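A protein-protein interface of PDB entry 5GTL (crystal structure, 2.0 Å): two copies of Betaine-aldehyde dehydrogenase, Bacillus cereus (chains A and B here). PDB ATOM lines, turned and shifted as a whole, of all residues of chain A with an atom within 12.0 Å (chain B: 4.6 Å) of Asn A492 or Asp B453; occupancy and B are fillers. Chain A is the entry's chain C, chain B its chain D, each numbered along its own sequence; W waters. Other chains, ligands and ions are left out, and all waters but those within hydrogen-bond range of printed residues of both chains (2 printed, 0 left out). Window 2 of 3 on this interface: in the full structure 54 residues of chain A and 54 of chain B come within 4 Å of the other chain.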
ATOM      1  N   ILE A 143     -25.827 -14.067  11.045  1.00  0.00           N
ATOM      2  CA  ILE A 143     -24.466 -14.449  11.193  1.00  0.00           C
ATOM      3  C   ILE A 143     -24.148 -14.965  12.561  1.00  0.00           C
ATOM      4  O   ILE A 143     -24.181 -14.251  13.499  1.00  0.00           O
ATOM      5  CB  ILE A 143     -23.543 -13.265  10.812  1.00  0.00           C
ATOM      6  CG1 ILE A 143     -24.108 -12.516   9.601  1.00  0.00           C
ATOM      7  CG2 ILE A 143     -22.129 -13.748  10.594  1.00  0.00           C
ATOM      8  CD1 ILE A 143     -23.396 -11.253   9.157  1.00  0.00           C
ATOM      9  N   ILE A 145     -21.984 -15.687  15.330  1.00  0.00           N
ATOM     10  CA  ILE A 145     -20.696 -15.279  15.770  1.00  0.00           C
ATOM     11  C   ILE A 145     -20.485 -15.622  17.197  1.00  0.00           C
ATOM     12  O   ILE A 145     -19.519 -16.215  17.517  1.00  0.00           O
ATOM     13  CB  ILE A 145     -20.484 -13.765  15.563  1.00  0.00           C
ATOM     14  CG1 ILE A 145     -20.850 -13.371  14.149  1.00  0.00           C
ATOM     15  CG2 ILE A 145     -19.093 -13.367  15.958  1.00  0.00           C
ATOM     16  CD1 ILE A 145     -20.426 -11.991  13.739  1.00  0.00           C
ATOM     17  N   SER A 146     -21.440 -15.250  18.019  1.00  0.00           N
ATOM     18  CA  SER A 146     -21.316 -15.367  19.469  1.00  0.00           C
ATOM     19  C   SER A 146     -22.689 -15.573  20.097  1.00  0.00           C
ATOM     20  O   SER A 146     -23.680 -15.027  19.631  1.00  0.00           O
ATOM     21  CB  SER A 146     -20.731 -14.065  19.996  1.00  0.00           C
ATOM     22  OG  SER A 146     -20.917 -13.972  21.387  1.00  0.00           O
ATOM     23  N   LYS A 147     -22.757 -16.306  21.191  1.00  0.00           N
ATOM     24  CA  LYS A 147     -24.036 -16.463  21.885  1.00  0.00           C
ATOM     25  C   LYS A 147     -24.526 -15.116  22.434  1.00  0.00           C
ATOM     26  O   LYS A 147     -25.687 -15.020  22.752  1.00  0.00           O
ATOM     27  CB  LYS A 147     -23.979 -17.518  22.987  1.00  0.00           C
ATOM     28  CG  LYS A 147     -23.510 -18.914  22.524  1.00  0.00           C
ATOM     29  CD  LYS A 147     -24.065 -19.337  21.141  1.00  0.00           C
ATOM     30  CE  LYS A 147     -23.470 -20.627  20.592  1.00  0.00           C
ATOM     31  NZ  LYS A 147     -24.169 -21.843  21.104  1.00  0.00           N
ATOM     32  N   ASP A 148     -23.667 -14.122  22.553  1.00  0.00           N
ATOM     33  CA  ASP A 148     -24.088 -12.870  23.146  1.00  0.00           C
ATOM     34  C   ASP A 148     -24.761 -11.865  22.250  1.00  0.00           C
ATOM     35  O   ASP A 148     -25.217 -10.862  22.713  1.00  0.00           O
ATOM     36  CB  ASP A 148     -22.934 -12.166  23.816  1.00  0.00           C
ATOM     37  CG  ASP A 148     -22.281 -12.982  24.872  1.00  0.00           C
ATOM     38  OD1 ASP A 148     -22.908 -13.795  25.515  1.00  0.00           O
ATOM     39  OD2 ASP A 148     -21.113 -12.781  25.014  1.00  0.00           O
ATOM     40  N   TYR A 149     -24.764 -12.129  20.958  1.00  0.00           N
ATOM     41  CA  TYR A 149     -25.341 -11.248  19.982  1.00  0.00           C
ATOM     42  C   TYR A 149     -26.113 -11.919  18.845  1.00  0.00           C
ATOM     43  O   TYR A 149     -25.765 -12.962  18.409  1.00  0.00           O
ATOM     44  CB  TYR A 149     -24.218 -10.454  19.284  1.00  0.00           C
ATOM     45  CG  TYR A 149     -23.407  -9.627  20.194  1.00  0.00           C
ATOM     46  CD1 TYR A 149     -23.728  -8.327  20.435  1.00  0.00           C
ATOM     47  CD2 TYR A 149     -22.333 -10.149  20.827  1.00  0.00           C
ATOM     48  CE1 TYR A 149     -23.004  -7.577  21.300  1.00  0.00           C
ATOM     49  CE2 TYR A 149     -21.594  -9.407  21.699  1.00  0.00           C
ATOM     50  CZ  TYR A 149     -21.944  -8.124  21.928  1.00  0.00           C
ATOM     51  OH  TYR A 149     -21.225  -7.399  22.807  1.00  0.00           O
ATOM     52  N   LEU A 150     -27.152 -11.261  18.379  1.00  0.00           N
ATOM     53  CA  LEU A 150     -27.878 -11.654  17.197  1.00  0.00           C
ATOM     54  C   LEU A 150     -27.260 -10.721  16.191  1.00  0.00           C
ATOM     55  O   LEU A 150     -27.295  -9.553  16.404  1.00  0.00           O
ATOM     56  CB  LEU A 150     -29.366 -11.394  17.296  1.00  0.00           C
ATOM     57  CG  LEU A 150     -30.133 -11.035  16.036  1.00  0.00           C
ATOM     58  CD1 LEU A 150     -29.945 -12.080  14.977  1.00  0.00           C
ATOM     59  CD2 LEU A 150     -31.599 -10.791  16.264  1.00  0.00           C
ATOM     60  N   ASN A 151     -26.677 -11.237  15.124  1.00  0.00           N
ATOM     61  CA  ASN A 151     -26.063 -10.428  14.121  1.00  0.00           C
ATOM     62  C   ASN A 151     -26.849 -10.673  12.825  1.00  0.00           C
ATOM     63  O   ASN A 151     -27.055 -11.799  12.458  1.00  0.00           O
ATOM     64  CB  ASN A 151     -24.599 -10.824  13.843  1.00  0.00           C
ATOM     65  CG  ASN A 151     -23.619 -10.459  14.954  1.00  0.00           C
ATOM     66  OD1 ASN A 151     -23.553 -11.111  15.916  1.00  0.00           O
ATOM     67  ND2 ASN A 151     -22.843  -9.442  14.756  1.00  0.00           N
ATOM     68  N   TYR A 152     -27.246  -9.617  12.150  1.00  0.00           N
ATOM     69  CA  TYR A 152     -27.941  -9.756  10.844  1.00  0.00           C
ATOM     70  C   TYR A 152     -27.703  -8.589   9.947  1.00  0.00           C
ATOM     71  O   TYR A 152     -27.419  -7.503  10.454  1.00  0.00           O
ATOM     72  CB  TYR A 152     -29.451  -9.887  11.019  1.00  0.00           C
ATOM     73  CG  TYR A 152     -30.265  -8.739  11.582  1.00  0.00           C
ATOM     74  CD1 TYR A 152     -30.403  -8.543  12.991  1.00  0.00           C
ATOM     75  CD2 TYR A 152     -30.933  -7.845  10.744  1.00  0.00           C
ATOM     76  CE1 TYR A 152     -31.214  -7.520  13.492  1.00  0.00           C
ATOM     77  CE2 TYR A 152     -31.713  -6.821  11.248  1.00  0.00           C
ATOM     78  CZ  TYR A 152     -31.842  -6.686  12.634  1.00  0.00           C
ATOM     79  OH  TYR A 152     -32.621  -5.688  13.019  1.00  0.00           O
ATOM     80  N   SER A 488     -25.327  -3.712   8.795  1.00  0.00           N
ATOM     81  CA  SER A 488     -25.016  -4.769   9.741  1.00  0.00           C
ATOM     82  C   SER A 488     -25.508  -4.324  11.097  1.00  0.00           C
ATOM     83  O   SER A 488     -25.080  -3.306  11.617  1.00  0.00           O
ATOM     84  CB  SER A 488     -23.496  -5.086   9.729  1.00  0.00           C
ATOM     85  OG  SER A 488     -23.110  -5.795  10.879  1.00  0.00           O
ATOM     86  N   VAL A 489     -26.451  -5.088  11.645  1.00  0.00           N
ATOM     87  CA  VAL A 489     -27.075  -4.798  12.886  1.00  0.00           C
ATOM     88  C   VAL A 489     -26.557  -5.828  13.834  1.00  0.00           C
ATOM     89  O   VAL A 489     -26.538  -7.002  13.485  1.00  0.00           O
ATOM     90  CB  VAL A 489     -28.640  -4.904  12.847  1.00  0.00           C
ATOM     91  CG1 VAL A 489     -29.238  -4.515  14.197  1.00  0.00           C
ATOM     92  CG2 VAL A 489     -29.212  -4.094  11.698  1.00  0.00           C
ATOM     93  N   TRP A 490     -26.204  -5.363  15.034  1.00  0.00           N
ATOM     94  CA  TRP A 490     -25.760  -6.148  16.150  1.00  0.00           C
ATOM     95  C   TRP A 490     -26.686  -5.848  17.271  1.00  0.00           C
ATOM     96  O   TRP A 490     -26.857  -4.684  17.570  1.00  0.00           O
ATOM     97  CB  TRP A 490     -24.394  -5.690  16.653  1.00  0.00           C
ATOM     98  CG  TRP A 490     -23.268  -5.855  15.807  1.00  0.00           C
ATOM     99  CD1 TRP A 490     -23.058  -5.262  14.594  1.00  0.00           C
ATOM    100  CD2 TRP A 490     -22.096  -6.605  16.106  1.00  0.00           C
ATOM    101  NE1 TRP A 490     -21.840  -5.632  14.115  1.00  0.00           N
ATOM    102  CE2 TRP A 490     -21.241  -6.483  14.999  1.00  0.00           C
ATOM    103  CE3 TRP A 490     -21.714  -7.443  17.170  1.00  0.00           C
ATOM    104  CZ2 TRP A 490     -19.969  -7.109  14.950  1.00  0.00           C
ATOM    105  CZ3 TRP A 490     -20.458  -8.099  17.105  1.00  0.00           C
ATOM    106  CH2 TRP A 490     -19.607  -7.913  16.012  1.00  0.00           C
ATOM    107  N   VAL A 491     -27.336  -6.895  17.821  1.00  0.00           N
ATOM    108  CA  VAL A 491     -28.206  -6.836  18.964  1.00  0.00           C
ATOM    109  C   VAL A 491     -27.574  -7.561  20.153  1.00  0.00           C
ATOM    110  O   VAL A 491     -27.464  -8.806  20.238  1.00  0.00           O
ATOM    111  CB  VAL A 491     -29.621  -7.448  18.710  1.00  0.00           C
ATOM    112  CG1 VAL A 491     -30.589  -6.998  19.792  1.00  0.00           C
ATOM    113  CG2 VAL A 491     -30.147  -7.054  17.361  1.00  0.00           C
ATOM    114  N   ASN A 492     -27.175  -6.753  21.115  1.00  0.00           N
ATOM    115  CA  ASN A 492     -26.673  -7.291  22.359  1.00  0.00           C
ATOM    116  C   ASN A 492     -27.797  -8.038  23.033  1.00  0.00           C
ATOM    117  O   ASN A 492     -28.860  -7.476  23.335  1.00  0.00           O
ATOM    118  CB  ASN A 492     -26.187  -6.154  23.220  1.00  0.00           C
ATOM    119  CG  ASN A 492     -25.599  -6.643  24.523  1.00  0.00           C
ATOM    120  OD1 ASN A 492     -26.222  -7.412  25.246  1.00  0.00           O
ATOM    121  ND2 ASN A 492     -24.408  -6.236  24.797  1.00  0.00           N
ATOM    122  N   ILE A 493     -27.600  -9.334  23.242  1.00  0.00           N
ATOM    123  CA  ILE A 493     -28.556 -10.141  24.004  1.00  0.00           C
ATOM    124  C   ILE A 493     -27.870 -10.861  25.181  1.00  0.00           C
ATOM    125  O   ILE A 493     -28.293 -11.949  25.597  1.00  0.00           O
ATOM    126  CB  ILE A 493     -29.291 -11.157  23.096  1.00  0.00           C
ATOM    127  CG1 ILE A 493     -28.314 -12.168  22.452  1.00  0.00           C
ATOM    128  CG2 ILE A 493     -30.080 -10.411  22.032  1.00  0.00           C
ATOM    129  CD1 ILE A 493     -28.958 -13.089  21.429  1.00  0.00           C
ATOM    130  N   LYS A 494     -26.813 -10.250  25.717  1.00  0.00           N
ATOM    131  CA  LYS A 494     -26.097 -10.817  26.903  1.00  0.00           C
ATOM    132  C   LYS A 494     -26.987 -10.771  28.124  1.00  0.00           C
ATOM    133  O   LYS A 494     -27.496  -9.697  28.370  1.00  0.00           O
ATOM    134  CB  LYS A 494     -24.837 -10.000  27.219  1.00  0.00           C
ATOM    135  CG  LYS A 494     -23.598 -10.627  26.687  1.00  0.00           C
ATOM    136  CD  LYS A 494     -22.306  -9.925  27.083  1.00  0.00           C
ATOM    137  CE  LYS A 494     -22.027  -8.677  26.264  1.00  0.00           C
ATOM    138  NZ  LYS A 494     -20.566  -8.482  26.036  1.00  0.00           N
ATOM    139  OXT LYS A 494     -27.232 -11.747  28.843  1.00  0.00           O
ATOM    140  N   GLY B 428     -25.142   3.941  17.123  1.00  0.00           N
ATOM    141  CA  GLY B 428     -25.504   3.244  18.310  1.00  0.00           C
ATOM    142  C   GLY B 428     -26.902   3.615  18.803  1.00  0.00           C
ATOM    143  O   GLY B 428     -27.342   4.807  18.748  1.00  0.00           O
ATOM    144  N   TRP B 430     -29.515   2.918  22.147  1.00  0.00           N
ATOM    145  CA  TRP B 430     -29.685   2.391  23.480  1.00  0.00           C
ATOM    146  C   TRP B 430     -31.135   2.540  23.873  1.00  0.00           C
ATOM    147  O   TRP B 430     -31.650   3.667  24.002  1.00  0.00           O
ATOM    148  CB  TRP B 430     -28.737   3.108  24.463  1.00  0.00           C
ATOM    149  CG  TRP B 430     -27.295   2.964  24.065  1.00  0.00           C
ATOM    150  CD1 TRP B 430     -26.606   3.729  23.190  1.00  0.00           C
ATOM    151  CD2 TRP B 430     -26.396   1.990  24.538  1.00  0.00           C
ATOM    152  NE1 TRP B 430     -25.320   3.273  23.054  1.00  0.00           N
ATOM    153  CE2 TRP B 430     -25.164   2.202  23.880  1.00  0.00           C
ATOM    154  CE3 TRP B 430     -26.505   0.959  25.473  1.00  0.00           C
ATOM    155  CZ2 TRP B 430     -24.039   1.417  24.122  1.00  0.00           C
ATOM    156  CZ3 TRP B 430     -25.412   0.169  25.698  1.00  0.00           C
ATOM    157  CH2 TRP B 430     -24.187   0.404  25.041  1.00  0.00           C
ATOM    158  N   TRP B 450     -25.327  -0.788  16.169  1.00  0.00           N
ATOM    159  CA  TRP B 450     -25.309  -1.568  17.362  1.00  0.00           C
ATOM    160  C   TRP B 450     -26.473  -1.167  18.273  1.00  0.00           C
ATOM    161  O   TRP B 450     -26.673   0.029  18.506  1.00  0.00           O
ATOM    162  CB  TRP B 450     -23.978  -1.288  18.087  1.00  0.00           C
ATOM    163  CG  TRP B 450     -22.742  -1.622  17.307  1.00  0.00           C
ATOM    164  CD1 TRP B 450     -22.185  -2.858  17.122  1.00  0.00           C
ATOM    165  CD2 TRP B 450     -21.839  -0.690  16.697  1.00  0.00           C
ATOM    166  NE1 TRP B 450     -21.012  -2.741  16.429  1.00  0.00           N
ATOM    167  CE2 TRP B 450     -20.784  -1.415  16.156  1.00  0.00           C
ATOM    168  CE3 TRP B 450     -21.818   0.701  16.592  1.00  0.00           C
ATOM    169  CZ2 TRP B 450     -19.717  -0.819  15.535  1.00  0.00           C
ATOM    170  CZ3 TRP B 450     -20.763   1.294  15.939  1.00  0.00           C
ATOM    171  CH2 TRP B 450     -19.738   0.540  15.404  1.00  0.00           C
ATOM    172  N   ILE B 451     -27.269  -2.146  18.710  1.00  0.00           N
ATOM    173  CA  ILE B 451     -28.392  -1.921  19.602  1.00  0.00           C
ATOM    174  C   ILE B 451     -27.913  -2.363  20.961  1.00  0.00           C
ATOM    175  O   ILE B 451     -27.755  -3.570  21.269  1.00  0.00           O
ATOM    176  CB  ILE B 451     -29.680  -2.685  19.225  1.00  0.00           C
ATOM    177  CG1 ILE B 451     -30.056  -2.398  17.761  1.00  0.00           C
ATOM    178  CG2 ILE B 451     -30.803  -2.368  20.202  1.00  0.00           C
ATOM    179  CD1 ILE B 451     -31.262  -3.144  17.260  1.00  0.00           C
ATOM    180  N   ASN B 452     -27.733  -1.384  21.811  1.00  0.00           N
ATOM    181  CA  ASN B 452     -27.286  -1.609  23.197  1.00  0.00           C
ATOM    182  C   ASN B 452     -25.828  -2.075  23.256  1.00  0.00           C
ATOM    183  O   ASN B 452     -25.484  -2.925  24.002  1.00  0.00           O
ATOM    184  CB  ASN B 452     -28.230  -2.534  23.933  1.00  0.00           C
ATOM    185  CG  ASN B 452     -29.642  -1.939  24.116  1.00  0.00           C
ATOM    186  OD1 ASN B 452     -29.797  -0.758  24.264  1.00  0.00           O
ATOM    187  ND2 ASN B 452     -30.648  -2.788  24.162  1.00  0.00           N
ATOM    188  N   ASP B 453     -25.008  -1.474  22.429  1.00  0.00           N
ATOM    189  CA  ASP B 453     -23.593  -1.716  22.354  1.00  0.00           C
ATOM    190  C   ASP B 453     -22.951  -0.687  21.473  1.00  0.00           C
ATOM    191  O   ASP B 453     -23.600   0.190  21.015  1.00  0.00           O
ATOM    192  CB  ASP B 453     -23.239  -3.135  21.996  1.00  0.00           C
ATOM    193  CG  ASP B 453     -22.144  -3.695  22.904  1.00  0.00           C
ATOM    194  OD1 ASP B 453     -21.155  -3.035  23.047  1.00  0.00           O
ATOM    195  OD2 ASP B 453     -22.267  -4.771  23.448  1.00  0.00           O
ATOM    196  N   TYR B 454     -21.667  -0.797  21.278  1.00  0.00           N
ATOM    197  CA  TYR B 454     -20.958   0.126  20.462  1.00  0.00           C
ATOM    198  C   TYR B 454     -19.551  -0.375  20.100  1.00  0.00           C
ATOM    199  O   TYR B 454     -18.969  -1.066  20.846  1.00  0.00           O
ATOM    200  CB  TYR B 454     -20.915   1.519  21.085  1.00  0.00           C
ATOM    201  CG  TYR B 454     -20.742   2.544  20.035  1.00  0.00           C
ATOM    202  CD1 TYR B 454     -19.512   2.868  19.572  1.00  0.00           C
ATOM    203  CD2 TYR B 454     -21.838   3.105  19.432  1.00  0.00           C
ATOM    204  CE1 TYR B 454     -19.362   3.765  18.568  1.00  0.00           C
ATOM    205  CE2 TYR B 454     -21.717   3.985  18.431  1.00  0.00           C
ATOM    206  CZ  TYR B 454     -20.488   4.320  17.995  1.00  0.00           C
ATOM    207  OH  TYR B 454     -20.427   5.164  17.000  1.00  0.00           O
ATOM    208  N   LEU B 456     -18.307  -2.711  18.055  1.00  0.00           N
ATOM    209  CA  LEU B 456     -18.013  -4.128  17.865  1.00  0.00           C
ATOM    210  C   LEU B 456     -17.726  -4.469  16.378  1.00  0.00           C
ATOM    211  O   LEU B 456     -18.493  -4.112  15.510  1.00  0.00           O
ATOM    212  CB  LEU B 456     -19.178  -5.002  18.371  1.00  0.00           C
ATOM    213  CG  LEU B 456     -19.748  -4.727  19.743  1.00  0.00           C
ATOM    214  CD1 LEU B 456     -20.972  -5.601  19.917  1.00  0.00           C
ATOM    215  CD2 LEU B 456     -18.735  -5.021  20.837  1.00  0.00           C
HETATM  216  O   HOH W   1     -29.879  -5.178  22.607  1.00  0.00           O
HETATM  217  O   HOH W   2     -21.341  -5.194  26.198  1.00  0.00           O
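Among the printed residues, pairs that only touch across the chains: Tyr A149 with Leu B456 (3.2 Å), Trp A490 with Leu B456 (3.4 Å), Asn A492 with Asn B452 (3.4 Å), Trp A490 with Trp B450 (3.4 Å) and Val A489 with Ile B451 (3.9 Å).
The backbone NH of Ile B451 sits at hydrogen-bond distance from the backbone carbonyl oxygen of Trp A490 (2.8 Å).
The side-chain hydroxyl (OH) of Tyr A149 is in hydrogen-bond range of the side-chain carboxylate (OD2) of Asp B453 (2.9 Å).
The side-chain carboxylate (OD2) of Asp B453 is in hydrogen-bond range of the side-chain amide nitrogen (ND2) of Asn A492, 2.9 Å away.
O of Ile B451 sits at hydrogen-bond distance from N of Asn A492 (3.2 Å).
Of the 16 printed residues of chain A, 4 touch a printed residue of chain B.
Printed residues of chain A that touch a printed residue of chain B: Tyr A149, Val A489, Trp A490 and Asn A492.
Hydrophobic or aromatic side chains of chain A within 4 Å of the printed part of chain B: Tyr A149, Val A489 and Trp A490.
Along chain A the printed residues that touch a printed residue of chain B span positions 149 to 492.
Of the 8 printed residues of chain B, 5 touch a printed residue of chain A.
Water W1 lies within hydrogen-bond range of the backbone carbonyl oxygen (O) of Asn A492, the side-chain amide nitrogen (ND2) of Asn B452 and the backbone carbonyl oxygen (O) of Ile B451.
Water W2 lies within hydrogen-bond range of the side-chain carboxylate of Asp B453 (2.9 Å) and the side-chain amino group of Lys A494 (3.4 Å).
No position is printed for both chains.
Of the 9 pairs that touch across the chains among the printed residues, none has its exchanged pair printed and touching as well.
Ile A145 touches none of the printed residues of chain B.
Of the printed residues of chain B, Tyr A149 touches Asp B453 and Leu B456.
Printed residues of chain B within 4 Å of Val A489: Ile B451 (3.9 Å).
Of the printed residues of chain B, Trp A490 touches Trp B450, Ile B451 and Leu B456.
Asn A492 touches three residues of chain B.
No residue of chain A comes within 4 Å of Gly B428.
Trp B450 touches just one residue of chain A: Trp A490 (3.4 Å).
Of the printed residues of chain A, Ile B451 touches Val A489 (3.9 Å), Trp A490 (2.8 Å) and Asn A492 (3.2 Å).
Asn B452 touches one residue of chain A.
Of chain A, only Tyr A149 and Asn A492 come within 4 Å of Asp B453.
No residue of chain A comes within 4 Å of Tyr B454.
Of the printed residues of chain A, Leu B456 touches Tyr A149 (3.2 Å) and Trp A490 (3.4 Å).
The nearest printed residue of chain B that does not touch Asn A492 is Leu B456 (6.0 Å).
The nearest printed residue of chain B that does not touch Tyr A149 is Asn B452 (5.9 Å).
O of Leu B456 is in hydrogen-bond range of NE1 of Trp B450, at 3.0 Å.
The side-chain hydroxyl (OG) of Ser A488 sits at hydrogen-bond distance from the indole nitrogen (NE1) of Trp A490, 3.5 Å away.
The backbone carbonyl oxygen of Tyr A152 is in hydrogen-bond range of the backbone NH of Val A489, at 2.9 Å.
The side-chain amino group (NZ) of Lys A494 lies within hydrogen-bond range of the side-chain hydroxyl (OH) of Tyr A149, 3.5 Å away.
OD1 of Asn A492 lies within hydrogen-bond range of N of Lys A494, at 2.9 Å.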
